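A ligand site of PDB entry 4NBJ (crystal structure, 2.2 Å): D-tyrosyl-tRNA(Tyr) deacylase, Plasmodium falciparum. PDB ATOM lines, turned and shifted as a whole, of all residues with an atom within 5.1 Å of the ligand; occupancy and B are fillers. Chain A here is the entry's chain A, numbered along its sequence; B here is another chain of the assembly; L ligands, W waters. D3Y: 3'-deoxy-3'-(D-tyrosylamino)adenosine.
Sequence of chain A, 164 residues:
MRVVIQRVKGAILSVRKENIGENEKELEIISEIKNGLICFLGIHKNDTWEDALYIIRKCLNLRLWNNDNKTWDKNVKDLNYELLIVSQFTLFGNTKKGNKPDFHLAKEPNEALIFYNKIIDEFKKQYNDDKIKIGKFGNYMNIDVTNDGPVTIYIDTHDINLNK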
ATOM      1  N   LEU A  41      11.329 -12.408   4.964  1.00  0.00           N
ATOM      2  CA  LEU A  41      11.091 -12.026   3.581  1.00  0.00           C
ATOM      3  C   LEU A  41      10.740 -13.214   2.677  1.00  0.00           C
ATOM      4  O   LEU A  41      11.534 -14.137   2.510  1.00  0.00           O
ATOM      5  CB  LEU A  41      12.353 -11.333   3.069  1.00  0.00           C
ATOM      6  CG  LEU A  41      12.303 -10.477   1.801  1.00  0.00           C
ATOM      7  CD1 LEU A  41      13.456  -9.473   1.819  1.00  0.00           C
ATOM      8  CD2 LEU A  41      12.427 -11.355   0.581  1.00  0.00           C
ATOM      9  N   GLY A  42       9.568 -13.159   2.065  1.00  0.00           N
ATOM     10  CA  GLY A  42       9.150 -14.194   1.117  1.00  0.00           C
ATOM     11  C   GLY A  42       9.176 -13.721  -0.339  1.00  0.00           C
ATOM     12  O   GLY A  42       8.554 -12.696  -0.695  1.00  0.00           O
ATOM     13  N   ILE A  43       9.908 -14.465  -1.182  1.00  0.00           N
ATOM     14  CA  ILE A  43      10.004 -14.182  -2.627  1.00  0.00           C
ATOM     15  C   ILE A  43       8.967 -15.005  -3.400  1.00  0.00           C
ATOM     16  O   ILE A  43       8.970 -16.233  -3.353  1.00  0.00           O
ATOM     17  CB  ILE A  43      11.439 -14.428  -3.129  1.00  0.00           C
ATOM     18  CG1 ILE A  43      12.404 -13.559  -2.301  1.00  0.00           C
ATOM     19  CG2 ILE A  43      11.579 -14.139  -4.628  1.00  0.00           C
ATOM     20  CD1 ILE A  43      13.859 -13.884  -2.515  1.00  0.00           C
ATOM     21  N   SER A  87      15.244 -15.189   5.233  1.00  0.00           N
ATOM     22  CA  SER A  87      14.446 -15.756   4.170  1.00  0.00           C
ATOM     23  C   SER A  87      13.393 -16.705   4.718  1.00  0.00           C
ATOM     24  O   SER A  87      13.729 -17.611   5.491  1.00  0.00           O
ATOM     25  CB  SER A  87      15.355 -16.493   3.168  1.00  0.00           C
ATOM     26  OG  SER A  87      16.263 -17.355   3.837  1.00  0.00           O
ATOM     27  N   GLN A  88      12.136 -16.499   4.322  1.00  0.00           N
ATOM     28  CA  GLN A  88      10.965 -17.247   4.818  1.00  0.00           C
ATOM     29  C   GLN A  88       9.988 -17.568   3.696  1.00  0.00           C
ATOM     30  O   GLN A  88       9.176 -16.715   3.324  1.00  0.00           O
ATOM     31  CB  GLN A  88      10.187 -16.411   5.863  1.00  0.00           C
ATOM     32  CG  GLN A  88      10.630 -16.527   7.303  1.00  0.00           C
ATOM     33  CD  GLN A  88      10.101 -17.785   7.990  1.00  0.00           C
ATOM     34  OE1 GLN A  88       9.283 -17.712   8.905  1.00  0.00           O
ATOM     35  NE2 GLN A  88      10.577 -18.949   7.548  1.00  0.00           N
ATOM     36  N   PHE A  89       9.988 -18.791   3.181  1.00  0.00           N
ATOM     37  CA  PHE A  89       9.015 -19.116   2.126  1.00  0.00           C
ATOM     38  C   PHE A  89       7.614 -19.466   2.654  1.00  0.00           C
ATOM     39  O   PHE A  89       6.657 -19.582   1.887  1.00  0.00           O
ATOM     40  CB  PHE A  89       9.570 -20.180   1.165  1.00  0.00           C
ATOM     41  CG  PHE A  89       9.308 -21.611   1.562  1.00  0.00           C
ATOM     42  CD1 PHE A  89       9.072 -22.574   0.583  1.00  0.00           C
ATOM     43  CD2 PHE A  89       9.326 -22.009   2.886  1.00  0.00           C
ATOM     44  CE1 PHE A  89       8.830 -23.910   0.933  1.00  0.00           C
ATOM     45  CE2 PHE A  89       9.085 -23.334   3.245  1.00  0.00           C
ATOM     46  CZ  PHE A  89       8.841 -24.286   2.266  1.00  0.00           C
ATOM     47  N   THR A  90       7.521 -19.627   3.972  1.00  0.00           N
ATOM     48  CA  THR A  90       6.280 -19.996   4.650  1.00  0.00           C
ATOM     49  C   THR A  90       5.189 -18.954   4.530  1.00  0.00           C
ATOM     50  O   THR A  90       4.007 -19.267   4.656  1.00  0.00           O
ATOM     51  CB  THR A  90       6.505 -20.383   6.147  1.00  0.00           C
ATOM     52  OG1 THR A  90       7.019 -19.263   6.912  1.00  0.00           O
ATOM     53  CG2 THR A  90       7.486 -21.570   6.230  1.00  0.00           C
ATOM     54  N   ALA A 106       5.624 -19.820  -3.986  1.00  0.00           N
ATOM     55  CA  ALA A 106       7.021 -19.468  -3.703  1.00  0.00           C
ATOM     56  C   ALA A 106       7.931 -19.681  -4.912  1.00  0.00           C
ATOM     57  O   ALA A 106       7.758 -20.638  -5.682  1.00  0.00           O
ATOM     58  CB  ALA A 106       7.552 -20.241  -2.497  1.00  0.00           C
ATOM     59  N   LYS A 107       8.903 -18.784  -5.068  1.00  0.00           N
ATOM     60  CA  LYS A 107       9.926 -18.961  -6.086  1.00  0.00           C
ATOM     61  C   LYS A 107      10.823 -20.136  -5.705  1.00  0.00           C
ATOM     62  O   LYS A 107      11.194 -20.304  -4.527  1.00  0.00           O
ATOM     63  CB  LYS A 107      10.764 -17.700  -6.250  1.00  0.00           C
ATOM     64  CG  LYS A 107      11.917 -17.861  -7.218  1.00  0.00           C
ATOM     65  CD  LYS A 107      12.620 -16.552  -7.482  1.00  0.00           C
ATOM     66  CE  LYS A 107      12.143 -15.911  -8.761  1.00  0.00           C
ATOM     67  NZ  LYS A 107      10.737 -15.408  -8.670  1.00  0.00           N
ATOM     68  N   GLU A 108      11.163 -20.931  -6.716  1.00  0.00           N
ATOM     69  CA  GLU A 108      12.011 -22.102  -6.568  1.00  0.00           C
ATOM     70  C   GLU A 108      13.367 -21.693  -5.947  1.00  0.00           C
ATOM     71  O   GLU A 108      13.917 -20.627  -6.282  1.00  0.00           O
ATOM     72  CB  GLU A 108      12.118 -22.829  -7.924  1.00  0.00           C
ATOM     73  CG  GLU A 108      13.342 -23.720  -8.153  1.00  0.00           C
ATOM     74  CD  GLU A 108      14.428 -23.047  -8.971  1.00  0.00           C
ATOM     75  OE1 GLU A 108      14.341 -21.837  -9.285  1.00  0.00           O
ATOM     76  OE2 GLU A 108      15.404 -23.743  -9.322  1.00  0.00           O
ATOM     77  N   PRO A 109      13.881 -22.512  -5.019  1.00  0.00           N
ATOM     78  CA  PRO A 109      15.009 -22.137  -4.159  1.00  0.00           C
ATOM     79  C   PRO A 109      16.295 -21.671  -4.877  1.00  0.00           C
ATOM     80  O   PRO A 109      17.067 -20.897  -4.291  1.00  0.00           O
ATOM     81  CB  PRO A 109      15.269 -23.400  -3.336  1.00  0.00           C
ATOM     82  CG  PRO A 109      14.008 -24.195  -3.416  1.00  0.00           C
ATOM     83  CD  PRO A 109      13.394 -23.875  -4.744  1.00  0.00           C
ATOM     84  N   ALA A 112      15.506 -18.231  -6.082  1.00  0.00           N
ATOM     85  CA  ALA A 112      15.197 -17.439  -4.901  1.00  0.00           C
ATOM     86  C   ALA A 112      16.498 -16.982  -4.243  1.00  0.00           C
ATOM     87  O   ALA A 112      16.617 -15.832  -3.811  1.00  0.00           O
ATOM     88  CB  ALA A 112      14.333 -18.236  -3.941  1.00  0.00           C
ATOM     89  N   LYS A 136      20.655 -17.810   7.058  1.00  0.00           N
ATOM     90  CA  LYS A 136      21.313 -18.829   6.257  1.00  0.00           C
ATOM     91  C   LYS A 136      20.270 -19.490   5.397  1.00  0.00           C
ATOM     92  O   LYS A 136      19.670 -20.520   5.783  1.00  0.00           O
ATOM     93  CB  LYS A 136      21.997 -19.838   7.185  1.00  0.00           C
ATOM     94  CG  LYS A 136      23.333 -20.309   6.682  1.00  0.00           C
ATOM     95  CD  LYS A 136      23.804 -21.504   7.474  1.00  0.00           C
ATOM     96  CE  LYS A 136      24.881 -22.268   6.725  1.00  0.00           C
ATOM     97  NZ  LYS A 136      25.142 -23.535   7.445  1.00  0.00           N
ATOM     98  N   PHE A 137      20.030 -18.870   4.250  1.00  0.00           N
ATOM     99  CA  PHE A 137      19.097 -19.350   3.247  1.00  0.00           C
ATOM    100  C   PHE A 137      19.160 -20.865   3.116  1.00  0.00           C
ATOM    101  O   PHE A 137      20.236 -21.430   2.893  1.00  0.00           O
ATOM    102  CB  PHE A 137      19.428 -18.683   1.915  1.00  0.00           C
ATOM    103  CG  PHE A 137      18.333 -18.778   0.864  1.00  0.00           C
ATOM    104  CD1 PHE A 137      17.464 -17.725   0.670  1.00  0.00           C
ATOM    105  CD2 PHE A 137      18.209 -19.925   0.055  1.00  0.00           C
ATOM    106  CE1 PHE A 137      16.483 -17.798  -0.304  1.00  0.00           C
ATOM    107  CE2 PHE A 137      17.212 -19.993  -0.922  1.00  0.00           C
ATOM    108  CZ  PHE A 137      16.354 -18.930  -1.097  1.00  0.00           C
ATOM    109  N   GLY A 138      18.022 -21.513   3.282  1.00  0.00           N
ATOM    110  CA  GLY A 138      17.882 -22.957   3.110  1.00  0.00           C
ATOM    111  C   GLY A 138      18.219 -23.794   4.330  1.00  0.00           C
ATOM    112  O   GLY A 138      18.127 -24.994   4.282  1.00  0.00           O
ATOM    113  N   ASN A 139      18.579 -23.159   5.438  1.00  0.00           N
ATOM    114  CA  ASN A 139      18.964 -23.896   6.634  1.00  0.00           C
ATOM    115  C   ASN A 139      17.986 -23.714   7.768  1.00  0.00           C
ATOM    116  O   ASN A 139      17.416 -22.649   7.927  1.00  0.00           O
ATOM    117  CB  ASN A 139      20.342 -23.450   7.082  1.00  0.00           C
ATOM    118  CG  ASN A 139      21.431 -24.064   6.226  1.00  0.00           C
ATOM    119  OD1 ASN A 139      21.872 -25.175   6.500  1.00  0.00           O
ATOM    120  ND2 ASN A 139      21.870 -23.349   5.180  1.00  0.00           N
ATOM    121  N   TYR A 140      17.818 -24.749   8.583  1.00  0.00           N
ATOM    122  CA  TYR A 140      17.044 -24.634   9.819  1.00  0.00           C
ATOM    123  C   TYR A 140      17.636 -23.546  10.695  1.00  0.00           C
ATOM    124  O   TYR A 140      18.827 -23.524  10.918  1.00  0.00           O
ATOM    125  CB  TYR A 140      17.026 -25.950  10.599  1.00  0.00           C
ATOM    126  CG  TYR A 140      16.316 -25.815  11.943  1.00  0.00           C
ATOM    127  CD1 TYR A 140      14.926 -25.979  12.046  1.00  0.00           C
ATOM    128  CD2 TYR A 140      17.032 -25.509  13.107  1.00  0.00           C
ATOM    129  CE1 TYR A 140      14.278 -25.846  13.266  1.00  0.00           C
ATOM    130  CE2 TYR A 140      16.401 -25.381  14.330  1.00  0.00           C
ATOM    131  CZ  TYR A 140      15.032 -25.538  14.402  1.00  0.00           C
ATOM    132  OH  TYR A 140      14.413 -25.391  15.624  1.00  0.00           O
ATOM    133  N   MET A 141      16.808 -22.641  11.198  1.00  0.00           N
ATOM    134  CA  MET A 141      17.336 -21.586  12.068  1.00  0.00           C
ATOM    135  C   MET A 141      16.605 -21.514  13.389  1.00  0.00           C
ATOM    136  O   MET A 141      15.409 -21.769  13.462  1.00  0.00           O
ATOM    137  CB  MET A 141      17.314 -20.216  11.382  1.00  0.00           C
ATOM    138  CG  MET A 141      18.363 -20.013  10.296  1.00  0.00           C
ATOM    139  SD  MET A 141      18.019 -18.642   9.150  1.00  0.00           S
ATOM    140  CE  MET A 141      16.675 -19.323   8.172  1.00  0.00           C
ATOM    141  N   ASN B  66       6.689 -30.715  11.736  1.00  0.00           N
ATOM    142  CA  ASN B  66       7.057 -31.999  11.166  1.00  0.00           C
ATOM    143  C   ASN B  66       6.872 -33.110  12.186  1.00  0.00           C
ATOM    144  O   ASN B  66       6.723 -32.869  13.389  1.00  0.00           O
ATOM    145  CB  ASN B  66       8.506 -31.999  10.662  1.00  0.00           C
ATOM    146  CG  ASN B  66       8.765 -30.921   9.626  1.00  0.00           C
ATOM    147  OD1 ASN B  66       7.841 -30.444   8.944  1.00  0.00           O
ATOM    148  ND2 ASN B  66      10.024 -30.519   9.497  1.00  0.00           N
ATOM    149  N   THR B  71       6.562 -34.166   6.668  1.00  0.00           N
ATOM    150  CA  THR B  71       6.685 -32.716   6.697  1.00  0.00           C
ATOM    151  C   THR B  71       5.319 -32.041   6.877  1.00  0.00           C
ATOM    152  O   THR B  71       4.301 -32.571   6.413  1.00  0.00           O
ATOM    153  CB  THR B  71       7.422 -32.200   5.439  1.00  0.00           C
ATOM    154  OG1 THR B  71       7.965 -30.910   5.698  1.00  0.00           O
ATOM    155  CG2 THR B  71       6.514 -32.173   4.204  1.00  0.00           C
ATOM    156  N   TRP B  72       5.282 -30.893   7.578  1.00  0.00           N
ATOM    157  CA  TRP B  72       4.020 -30.143   7.789  1.00  0.00           C
ATOM    158  C   TRP B  72       2.868 -31.036   8.158  1.00  0.00           C
ATOM    159  O   TRP B  72       1.862 -31.108   7.422  1.00  0.00           O
ATOM    160  CB  TRP B  72       3.641 -29.351   6.530  1.00  0.00           C
ATOM    161  CG  TRP B  72       4.797 -28.521   6.071  1.00  0.00           C
ATOM    162  CD1 TRP B  72       5.657 -28.776   5.013  1.00  0.00           C
ATOM    163  CD2 TRP B  72       5.278 -27.264   6.665  1.00  0.00           C
ATOM    164  NE1 TRP B  72       6.610 -27.783   4.912  1.00  0.00           N
ATOM    165  CE2 TRP B  72       6.440 -26.846   5.878  1.00  0.00           C
ATOM    166  CE3 TRP B  72       4.881 -26.476   7.733  1.00  0.00           C
ATOM    167  CZ2 TRP B  72       7.160 -25.685   6.163  1.00  0.00           C
ATOM    168  CZ3 TRP B  72       5.614 -25.313   8.015  1.00  0.00           C
ATOM    169  CH2 TRP B  72       6.716 -24.925   7.238  1.00  0.00           C
ATOM    170  N   GLY B 149      12.510 -22.517  13.334  1.00  0.00           N
ATOM    171  CA  GLY B 149      12.376 -22.698  11.898  1.00  0.00           C
ATOM    172  C   GLY B 149      13.162 -21.657  11.111  1.00  0.00           C
ATOM    173  O   GLY B 149      14.153 -21.993  10.480  1.00  0.00           O
ATOM    174  N   PRO B 150      12.717 -20.388  11.142  1.00  0.00           N
ATOM    175  CA  PRO B 150      11.469 -19.890  11.709  1.00  0.00           C
ATOM    176  C   PRO B 150      10.306 -20.304  10.812  1.00  0.00           C
ATOM    177  O   PRO B 150      10.520 -20.717   9.666  1.00  0.00           O
ATOM    178  CB  PRO B 150      11.655 -18.386  11.637  1.00  0.00           C
ATOM    179  CG  PRO B 150      12.533 -18.198  10.430  1.00  0.00           C
ATOM    180  CD  PRO B 150      13.500 -19.324  10.490  1.00  0.00           C
ATOM    181  N   VAL B 151       9.097 -20.229  11.339  1.00  0.00           N
ATOM    182  CA  VAL B 151       7.898 -20.493  10.567  1.00  0.00           C
ATOM    183  C   VAL B 151       6.952 -19.351  10.840  1.00  0.00           C
ATOM    184  O   VAL B 151       6.565 -19.132  11.970  1.00  0.00           O
ATOM    185  CB  VAL B 151       7.254 -21.831  10.953  1.00  0.00           C
ATOM    186  CG1 VAL B 151       5.876 -21.996  10.327  1.00  0.00           C
ATOM    187  CG2 VAL B 151       8.152 -22.974  10.527  1.00  0.00           C
HETATM  188  CD1 D3Y L   1      12.179 -24.474   5.935  1.00  0.00           C
HETATM  189  CE1 D3Y L   1      12.042 -25.785   5.474  1.00  0.00           C
HETATM  190  CZ  D3Y L   1      11.171 -26.675   6.123  1.00  0.00           C
HETATM  191  OH  D3Y L   1      11.052 -27.944   5.665  1.00  0.00           O
HETATM  192  CE2 D3Y L   1      10.463 -26.241   7.248  1.00  0.00           C
HETATM  193  CD2 D3Y L   1      10.613 -24.929   7.705  1.00  0.00           C
HETATM  194  CG  D3Y L   1      11.474 -24.038   7.047  1.00  0.00           C
HETATM  195  CB  D3Y L   1      11.571 -22.609   7.605  1.00  0.00           C
HETATM  196  CA  D3Y L   1      12.590 -21.598   7.013  1.00  0.00           C
HETATM  197  N   D3Y L   1      14.004 -22.014   7.240  1.00  0.00           N
HETATM  198  C   D3Y L   1      12.321 -21.273   5.517  1.00  0.00           C
HETATM  199  O   D3Y L   1      11.255 -20.795   5.132  1.00  0.00           O
HETATM  200  N8  D3Y L   1      13.378 -21.528   4.754  1.00  0.00           N
HETATM  201  C3' D3Y L   1      13.451 -21.352   3.316  1.00  0.00           C
HETATM  202  C2' D3Y L   1      14.264 -20.102   2.996  1.00  0.00           C
HETATM  203  O2' D3Y L   1      15.448 -19.946   3.829  1.00  0.00           O
HETATM  204  C4' D3Y L   1      14.419 -22.407   2.803  1.00  0.00           C
HETATM  205  C5' D3Y L   1      13.851 -23.847   2.683  1.00  0.00           C
HETATM  206  O5' D3Y L   1      13.264 -24.038   1.394  1.00  0.00           O
HETATM  207  O4' D3Y L   1      14.912 -21.860   1.553  1.00  0.00           O
HETATM  208  C1' D3Y L   1      14.729 -20.446   1.578  1.00  0.00           C
HETATM  209  N9  D3Y L   1      13.745 -20.153   0.535  1.00  0.00           N
HETATM  210  C8  D3Y L   1      13.371 -21.000  -0.439  1.00  0.00           C
HETATM  211  N7  D3Y L   1      12.474 -20.398  -1.213  1.00  0.00           N
HETATM  212  C5  D3Y L   1      12.269 -19.179  -0.751  1.00  0.00           C
HETATM  213  C4  D3Y L   1      13.085 -19.005   0.366  1.00  0.00           C
HETATM  214  N3  D3Y L   1      13.071 -17.821   1.034  1.00  0.00           N
HETATM  215  C2  D3Y L   1      12.274 -16.831   0.613  1.00  0.00           C
HETATM  216  N1  D3Y L   1      11.494 -16.967  -0.467  1.00  0.00           N
HETATM  217  C6  D3Y L   1      11.462 -18.133  -1.159  1.00  0.00           C
HETATM  218  N6  D3Y L   1      10.700 -18.281  -2.228  1.00  0.00           N
HETATM  219  O   HOH W   1      12.726 -27.419   2.871  1.00  0.00           O
HETATM  220  O   HOH W   2      11.031 -27.282  10.431  1.00  0.00           O
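NE1 of Trp 72 of chain B sits close to OG1 of Thr 71 of chain B, at 3.5 Å. The backbone carbonyl oxygen of Gly 149 of chain B lies within hydrogen-bond range of the backbone NH of Met 141 (2.8 Å). O of Leu 41 lies within hydrogen-bond range of N of Gln 88 (3.0 Å). The backbone carbonyl oxygen of Ile 43 is in hydrogen-bond range of the backbone NH of Lys 107, at 3.1 Å. The side-chain amide oxygen (OD1) of Asn 66 of chain B sits at hydrogen-bond distance from the backbone NH (N) of Trp 72 of chain B, 2.9 Å away. OE1 of Gln 88 sits at hydrogen-bond distance from OG1 of Thr 90 (3.4 Å). The backbone carbonyl oxygen (O) of Pro 150 of chain B sits at hydrogen-bond distance from the side-chain amide nitrogen (NE2) of Gln 88, 2.8 Å away. The backbone carbonyl oxygen (O) of Phe 137 sits at hydrogen-bond distance from the side-chain amide nitrogen (ND2) of Asn 139 (3.4 Å).
The backbone carbonyl oxygen of Gly 149 of chain B lies within hydrogen-bond range of a nitrogen (N) of the ligand, at 3.2 Å. N6 of the ligand sits at hydrogen-bond distance from O of Lys 107 (3.1 Å). The backbone NH of Gly 138 sits at hydrogen-bond distance from an oxygen (O2') of the ligand (3.1 Å). The side-chain hydroxyl of Ser 87 sits at hydrogen-bond distance from an oxygen (O2') of the ligand (2.7 Å). The backbone carbonyl oxygen (O) of Ile 43 lies within hydrogen-bond range of a nitrogen (N6) of the ligand, at 2.9 Å. N of Ile 43 lies within hydrogen-bond range of N1 of the ligand, at 3.0 Å. An oxygen (O) of the ligand lies within hydrogen-bond range of the side-chain amide nitrogen (NE2) of Gln 88, 3.1 Å away. The backbone carbonyl oxygen (O) of Ser 87 lies within hydrogen-bond range of an oxygen (O2') of the ligand, at 3.3 Å. O of the ligand is in hydrogen-bond range of N of Phe 89, at 3.1 Å.
Merely in contact with the ligand: Pro 150 of chain B, Phe 137, Leu 41, Trp 72 of chain B, Asn 139, Ala 106, Met 141, Ala 112 and Gly 42. Hydrophobic or aromatic side chains that line the ligand: Ile 43, Phe 89, Ala 106, Ala 112, Phe 137, Met 141 and Trp 72 of chain B. Of the 24 residues printed, 16 come within 4 Å of the ligand.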
